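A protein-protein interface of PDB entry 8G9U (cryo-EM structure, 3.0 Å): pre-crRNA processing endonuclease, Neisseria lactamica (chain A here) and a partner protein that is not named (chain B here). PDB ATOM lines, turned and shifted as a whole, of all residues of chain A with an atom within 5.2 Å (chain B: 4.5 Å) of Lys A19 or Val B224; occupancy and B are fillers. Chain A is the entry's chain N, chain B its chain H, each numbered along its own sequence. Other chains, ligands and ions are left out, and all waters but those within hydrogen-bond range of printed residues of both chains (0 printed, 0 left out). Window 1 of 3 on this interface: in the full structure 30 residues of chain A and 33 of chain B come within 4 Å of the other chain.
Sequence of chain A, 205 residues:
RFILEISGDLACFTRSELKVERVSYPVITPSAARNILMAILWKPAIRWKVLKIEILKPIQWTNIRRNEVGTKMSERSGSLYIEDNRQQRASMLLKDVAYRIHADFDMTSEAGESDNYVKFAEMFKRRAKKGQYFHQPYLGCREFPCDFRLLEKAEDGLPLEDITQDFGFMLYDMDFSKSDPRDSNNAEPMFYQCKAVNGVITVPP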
ATOM      1  N   THR A  14       7.521 -21.502 -29.235  1.00  0.00           N
ATOM      2  CA  THR A  14       7.056 -22.607 -28.418  1.00  0.00           C
ATOM      3  C   THR A  14       7.789 -23.883 -28.770  1.00  0.00           C
ATOM      4  O   THR A  14       7.806 -24.300 -29.929  1.00  0.00           O
ATOM      5  CB  THR A  14       5.558 -22.796 -28.594  1.00  0.00           C
ATOM      6  OG1 THR A  14       4.875 -21.605 -28.191  1.00  0.00           O
ATOM      7  CG2 THR A  14       5.090 -23.935 -27.750  1.00  0.00           C
ATOM      8  N   ARG A  15       8.413 -24.482 -27.762  1.00  0.00           N
ATOM      9  CA  ARG A  15       9.051 -25.771 -27.936  1.00  0.00           C
ATOM     10  C   ARG A  15       8.036 -26.744 -28.495  1.00  0.00           C
ATOM     11  O   ARG A  15       6.887 -26.775 -28.051  1.00  0.00           O
ATOM     12  CB  ARG A  15       9.579 -26.279 -26.597  1.00  0.00           C
ATOM     13  CG  ARG A  15      10.684 -25.452 -26.012  1.00  0.00           C
ATOM     14  CD  ARG A  15      11.466 -26.205 -24.965  1.00  0.00           C
ATOM     15  NE  ARG A  15      12.870 -25.853 -25.063  1.00  0.00           N
ATOM     16  CZ  ARG A  15      13.772 -26.588 -25.695  1.00  0.00           C
ATOM     17  NH1 ARG A  15      15.032 -26.183 -25.753  1.00  0.00           N
ATOM     18  NH2 ARG A  15      13.415 -27.727 -26.268  1.00  0.00           N
ATOM     19  N   SER A  16       8.446 -27.520 -29.492  1.00  0.00           N
ATOM     20  CA  SER A  16       7.541 -28.526 -30.018  1.00  0.00           C
ATOM     21  C   SER A  16       7.025 -29.418 -28.903  1.00  0.00           C
ATOM     22  O   SER A  16       5.834 -29.734 -28.856  1.00  0.00           O
ATOM     23  CB  SER A  16       8.236 -29.351 -31.096  1.00  0.00           C
ATOM     24  OG  SER A  16       8.533 -28.557 -32.229  1.00  0.00           O
ATOM     25  N   GLU A  17       7.903 -29.810 -27.976  1.00  0.00           N
ATOM     26  CA  GLU A  17       7.489 -30.691 -26.888  1.00  0.00           C
ATOM     27  C   GLU A  17       6.398 -30.052 -26.046  1.00  0.00           C
ATOM     28  O   GLU A  17       5.340 -30.647 -25.818  1.00  0.00           O
ATOM     29  CB  GLU A  17       8.690 -31.060 -26.018  1.00  0.00           C
ATOM     30  CG  GLU A  17       9.453 -29.898 -25.395  1.00  0.00           C
ATOM     31  CD  GLU A  17      10.738 -29.564 -26.118  1.00  0.00           C
ATOM     32  OE1 GLU A  17      10.676 -29.215 -27.312  1.00  0.00           O
ATOM     33  OE2 GLU A  17      11.812 -29.640 -25.488  1.00  0.00           O
ATOM     34  N   LEU A  18       6.633 -28.837 -25.585  1.00  0.00           N
ATOM     35  CA  LEU A  18       5.699 -28.154 -24.711  1.00  0.00           C
ATOM     36  C   LEU A  18       4.874 -27.170 -25.529  1.00  0.00           C
ATOM     37  O   LEU A  18       4.966 -25.958 -25.386  1.00  0.00           O
ATOM     38  CB  LEU A  18       6.453 -27.471 -23.588  1.00  0.00           C
ATOM     39  CG  LEU A  18       7.243 -28.508 -22.810  1.00  0.00           C
ATOM     40  CD1 LEU A  18       8.490 -27.900 -22.258  1.00  0.00           C
ATOM     41  CD2 LEU A  18       6.372 -29.044 -21.709  1.00  0.00           C
ATOM     42  N   LYS A  19       4.059 -27.734 -26.411  1.00  0.00           N
ATOM     43  CA  LYS A  19       3.232 -26.919 -27.281  1.00  0.00           C
ATOM     44  C   LYS A  19       1.873 -26.627 -26.660  1.00  0.00           C
ATOM     45  O   LYS A  19       1.404 -25.489 -26.683  1.00  0.00           O
ATOM     46  CB  LYS A  19       3.066 -27.614 -28.626  1.00  0.00           C
ATOM     47  CG  LYS A  19       2.489 -26.741 -29.683  1.00  0.00           C
ATOM     48  CD  LYS A  19       2.526 -27.440 -30.995  1.00  0.00           C
ATOM     49  CE  LYS A  19       2.372 -26.432 -32.077  1.00  0.00           C
ATOM     50  NZ  LYS A  19       1.168 -25.613 -31.823  1.00  0.00           N
ATOM     51  N   VAL A  20       1.230 -27.647 -26.097  1.00  0.00           N
ATOM     52  CA  VAL A  20      -0.050 -27.439 -25.451  1.00  0.00           C
ATOM     53  C   VAL A  20       0.078 -26.592 -24.208  1.00  0.00           C
ATOM     54  O   VAL A  20      -0.910 -26.016 -23.752  1.00  0.00           O
ATOM     55  CB  VAL A  20      -0.667 -28.790 -25.105  1.00  0.00           C
ATOM     56  CG1 VAL A  20      -0.962 -29.511 -26.353  1.00  0.00           C
ATOM     57  CG2 VAL A  20       0.312 -29.590 -24.277  1.00  0.00           C
ATOM     58  N   GLU A  21       1.268 -26.519 -23.632  1.00  0.00           N
ATOM     59  CA  GLU A  21       1.539 -25.790 -22.403  1.00  0.00           C
ATOM     60  C   GLU A  21       2.686 -24.833 -22.627  1.00  0.00           C
ATOM     61  O   GLU A  21       3.667 -24.817 -21.884  1.00  0.00           O
ATOM     62  CB  GLU A  21       1.832 -26.733 -21.247  1.00  0.00           C
ATOM     63  CG  GLU A  21       0.617 -27.483 -20.743  1.00  0.00           C
ATOM     64  CD  GLU A  21      -0.635 -26.629 -20.690  1.00  0.00           C
ATOM     65  OE1 GLU A  21      -1.707 -27.129 -21.080  1.00  0.00           O
ATOM     66  OE2 GLU A  21      -0.567 -25.469 -20.244  1.00  0.00           O
ATOM     67  N   ARG A  22       2.537 -24.003 -23.658  1.00  0.00           N
ATOM     68  CA  ARG A  22       3.630 -23.381 -24.392  1.00  0.00           C
ATOM     69  C   ARG A  22       4.789 -23.003 -23.489  1.00  0.00           C
ATOM     70  O   ARG A  22       4.636 -22.235 -22.540  1.00  0.00           O
ATOM     71  CB  ARG A  22       3.108 -22.137 -25.116  1.00  0.00           C
ATOM     72  CG  ARG A  22       2.265 -22.441 -26.339  1.00  0.00           C
ATOM     73  CD  ARG A  22       1.520 -21.220 -26.849  1.00  0.00           C
ATOM     74  NE  ARG A  22       0.731 -21.531 -28.037  1.00  0.00           N
ATOM     75  CZ  ARG A  22       1.234 -21.637 -29.265  1.00  0.00           C
ATOM     76  NH1 ARG A  22       2.528 -21.457 -29.477  1.00  0.00           N
ATOM     77  NH2 ARG A  22       0.447 -21.929 -30.287  1.00  0.00           N
ATOM     78  N   ARG A  89      -4.004 -22.960 -22.218  1.00  0.00           N
ATOM     79  CA  ARG A  89      -2.615 -23.233 -22.534  1.00  0.00           C
ATOM     80  C   ARG A  89      -1.755 -22.286 -21.722  1.00  0.00           C
ATOM     81  O   ARG A  89      -1.858 -21.066 -21.867  1.00  0.00           O
ATOM     82  CB  ARG A  89      -2.342 -23.071 -24.022  1.00  0.00           C
ATOM     83  CG  ARG A  89      -3.052 -24.065 -24.879  1.00  0.00           C
ATOM     84  CD  ARG A  89      -2.785 -23.782 -26.329  1.00  0.00           C
ATOM     85  NE  ARG A  89      -1.435 -24.112 -26.740  1.00  0.00           N
ATOM     86  CZ  ARG A  89      -1.048 -24.138 -28.005  1.00  0.00           C
ATOM     87  NH1 ARG A  89      -1.916 -23.857 -28.962  1.00  0.00           N
ATOM     88  NH2 ARG A  89       0.198 -24.450 -28.312  1.00  0.00           N
ATOM     89  N   ALA B 222       4.318 -34.149 -22.260  1.00  0.00           N
ATOM     90  CA  ALA B 222       4.323 -33.561 -23.589  1.00  0.00           C
ATOM     91  C   ALA B 222       3.296 -34.316 -24.413  1.00  0.00           C
ATOM     92  O   ALA B 222       3.504 -35.483 -24.752  1.00  0.00           O
ATOM     93  CB  ALA B 222       5.708 -33.637 -24.220  1.00  0.00           C
ATOM     94  N   SER B 223       2.185 -33.661 -24.728  1.00  0.00           N
ATOM     95  CA  SER B 223       1.110 -34.332 -25.451  1.00  0.00           C
ATOM     96  C   SER B 223       0.293 -33.282 -26.176  1.00  0.00           C
ATOM     97  O   SER B 223      -0.476 -32.555 -25.542  1.00  0.00           O
ATOM     98  CB  SER B 223       0.236 -35.114 -24.503  1.00  0.00           C
ATOM     99  OG  SER B 223      -0.636 -34.225 -23.830  1.00  0.00           O
ATOM    100  N   VAL B 224       0.438 -33.224 -27.492  1.00  0.00           N
ATOM    101  CA  VAL B 224      -0.347 -32.316 -28.308  1.00  0.00           C
ATOM    102  C   VAL B 224      -1.532 -33.077 -28.872  1.00  0.00           C
ATOM    103  O   VAL B 224      -1.469 -33.609 -29.982  1.00  0.00           O
ATOM    104  CB  VAL B 224       0.526 -31.706 -29.417  1.00  0.00           C
ATOM    105  CG1 VAL B 224      -0.304 -30.963 -30.410  1.00  0.00           C
ATOM    106  CG2 VAL B 224       1.529 -30.766 -28.808  1.00  0.00           C
ATOM    107  N   ASN B 225      -2.623 -33.156 -28.125  1.00  0.00           N
ATOM    108  CA  ASN B 225      -3.807 -33.846 -28.630  1.00  0.00           C
ATOM    109  C   ASN B 225      -5.033 -32.978 -28.456  1.00  0.00           C
ATOM    110  O   ASN B 225      -5.809 -33.172 -27.520  1.00  0.00           O
ATOM    111  CB  ASN B 225      -3.999 -35.164 -27.968  1.00  0.00           C
ATOM    112  CG  ASN B 225      -5.091 -35.967 -28.621  1.00  0.00           C
ATOM    113  OD1 ASN B 225      -5.733 -35.517 -29.567  1.00  0.00           O
ATOM    114  ND2 ASN B 225      -5.292 -37.171 -28.140  1.00  0.00           N
ATOM    115  N   LEU B 226      -5.218 -32.064 -29.401  1.00  0.00           N
ATOM    116  CA  LEU B 226      -6.500 -31.451 -29.685  1.00  0.00           C
ATOM    117  C   LEU B 226      -6.432 -30.945 -31.110  1.00  0.00           C
ATOM    118  O   LEU B 226      -5.347 -30.762 -31.663  1.00  0.00           O
ATOM    119  CB  LEU B 226      -6.848 -30.338 -28.704  1.00  0.00           C
ATOM    120  CG  LEU B 226      -7.763 -30.877 -27.615  1.00  0.00           C
ATOM    121  CD1 LEU B 226      -8.002 -29.848 -26.581  1.00  0.00           C
ATOM    122  CD2 LEU B 226      -9.072 -31.326 -28.221  1.00  0.00           C
ATOM    123  N   PHE B 229      -3.978 -28.039 -31.365  1.00  0.00           N
ATOM    124  CA  PHE B 229      -2.640 -27.744 -30.917  1.00  0.00           C
ATOM    125  C   PHE B 229      -1.649 -28.320 -31.897  1.00  0.00           C
ATOM    126  O   PHE B 229      -0.490 -27.906 -31.903  1.00  0.00           O
ATOM    127  CB  PHE B 229      -2.379 -28.329 -29.526  1.00  0.00           C
ATOM    128  CG  PHE B 229      -3.359 -27.893 -28.492  1.00  0.00           C
ATOM    129  CD1 PHE B 229      -3.737 -26.579 -28.392  1.00  0.00           C
ATOM    130  CD2 PHE B 229      -3.903 -28.804 -27.619  1.00  0.00           C
ATOM    131  CE1 PHE B 229      -4.637 -26.192 -27.439  1.00  0.00           C
ATOM    132  CE2 PHE B 229      -4.790 -28.416 -26.663  1.00  0.00           C
ATOM    133  CZ  PHE B 229      -5.157 -27.109 -26.573  1.00  0.00           C
ATOM    134  N   GLU B 230      -2.095 -29.262 -32.720  1.00  0.00           N
ATOM    135  CA  GLU B 230      -1.269 -29.827 -33.769  1.00  0.00           C
ATOM    136  C   GLU B 230      -0.828 -28.731 -34.707  1.00  0.00           C
ATOM    137  O   GLU B 230      -1.647 -27.952 -35.196  1.00  0.00           O
ATOM    138  CB  GLU B 230      -2.045 -30.895 -34.528  1.00  0.00           C
ATOM    139  CG  GLU B 230      -2.988 -31.684 -33.657  1.00  0.00           C
ATOM    140  CD  GLU B 230      -3.928 -32.544 -34.461  1.00  0.00           C
ATOM    141  OE1 GLU B 230      -4.394 -33.571 -33.927  1.00  0.00           O
ATOM    142  OE2 GLU B 230      -4.196 -32.196 -35.630  1.00  0.00           O
ATOM    143  N   SER B 231       0.469 -28.669 -34.960  1.00  0.00           N
ATOM    144  CA  SER B 231       0.990 -27.566 -35.753  1.00  0.00           C
ATOM    145  C   SER B 231       0.823 -27.831 -37.244  1.00  0.00           C
ATOM    146  O   SER B 231      -0.004 -27.202 -37.906  1.00  0.00           O
ATOM    147  CB  SER B 231       2.455 -27.332 -35.400  1.00  0.00           C
ATOM    148  OG  SER B 231       3.211 -28.490 -35.691  1.00  0.00           O
ATOM    149  N   GLN B 236      -0.193 -35.224 -32.719  1.00  0.00           N
ATOM    150  CA  GLN B 236      -0.164 -35.840 -31.395  1.00  0.00           C
ATOM    151  C   GLN B 236       1.141 -36.574 -31.085  1.00  0.00           C
ATOM    152  O   GLN B 236       1.156 -37.738 -30.687  1.00  0.00           O
ATOM    153  CB  GLN B 236      -1.400 -36.750 -31.286  1.00  0.00           C
ATOM    154  CG  GLN B 236      -1.489 -37.749 -30.161  1.00  0.00           C
ATOM    155  CD  GLN B 236      -2.637 -38.676 -30.351  1.00  0.00           C
ATOM    156  OE1 GLN B 236      -3.457 -38.860 -29.459  1.00  0.00           O
ATOM    157  NE2 GLN B 236      -2.713 -39.270 -31.531  1.00  0.00           N
ATOM    158  N   ALA B 239       4.006 -33.797 -33.644  1.00  0.00           N
ATOM    159  CA  ALA B 239       4.188 -32.368 -33.455  1.00  0.00           C
ATOM    160  C   ALA B 239       5.485 -32.100 -32.722  1.00  0.00           C
ATOM    161  O   ALA B 239       6.127 -31.067 -32.937  1.00  0.00           O
ATOM    162  CB  ALA B 239       3.004 -31.780 -32.692  1.00  0.00           C
ATOM    163  N   PHE B 240       5.888 -33.030 -31.867  1.00  0.00           N
ATOM    164  CA  PHE B 240       7.168 -32.996 -31.172  1.00  0.00           C
ATOM    165  C   PHE B 240       7.832 -34.355 -31.318  1.00  0.00           C
ATOM    166  O   PHE B 240       7.701 -35.230 -30.455  1.00  0.00           O
ATOM    167  CB  PHE B 240       6.982 -32.564 -29.724  1.00  0.00           C
ATOM    168  CG  PHE B 240       5.869 -33.259 -29.009  1.00  0.00           C
ATOM    169  CD1 PHE B 240       4.592 -32.762 -29.082  1.00  0.00           C
ATOM    170  CD2 PHE B 240       6.095 -34.346 -28.210  1.00  0.00           C
ATOM    171  CE1 PHE B 240       3.565 -33.370 -28.420  1.00  0.00           C
ATOM    172  CE2 PHE B 240       5.058 -34.943 -27.544  1.00  0.00           C
ATOM    173  CZ  PHE B 240       3.799 -34.455 -27.656  1.00  0.00           C
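The side-chain amino group (NZ) of Lys A19 sits at hydrogen-bond distance from the backbone carbonyl oxygen (O) of Phe B229.
The backbone NH (N) of Gln B236 lies close to the backbone carbonyl oxygen (O) of Val B224, at 3.4 Å. OE2 of Glu A17 lies within salt-bridge range of NH2 of Arg A15, 2.6 Å away. NE of Arg A89 lies close to O of Lys A19, 3.2 Å away.
Among the printed residues, pairs that only touch across the chains: Ser A16 with Ala B239, Ser A16 with Phe B240, Glu A17 with Ala B222, Glu A17 with Phe B240, Lys A19 with Val B224, Lys A19 with Ser B231, Val A20 with Ser B223, Val A20 with Val B224, Val A20 with Phe B229 and Arg A89 with Phe B229.
Of chain A, only Lys A19 and Val A20 come within 4 Å of Val B224. Printed residues of chain B within 4 Å of Val A20: Ser B223, Val B224 and Phe B229. Printed residues of chain A within 4 Å of Ser B231: Lys A19. Of the printed residues of chain A, Ser B223 touches Val A20. Printed residues of chain B within 4 Å of Arg A89: Phe B229 (3.2 Å). Of the printed residues of chain A, Phe B240 touches Ser A16 (3.2 Å) and Glu A17 (3.4 Å). Gln B236 touches none of the printed residues of chain A. Glu A21 touches none of the printed residues of chain B. The nearest residue of chain A that does not touch Val B224 is Ser A16 (4.4 Å).
Of the 10 printed residues of chain A, 5 touch a printed residue of chain B. Hydrophobic or aromatic side chains of chain A within 4 Å of the printed part of chain B: Val A20. Along chain A the printed residues that touch a printed residue of chain B span positions 16 to 89. Among the printed residues, 11 pairs touch across the chains.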
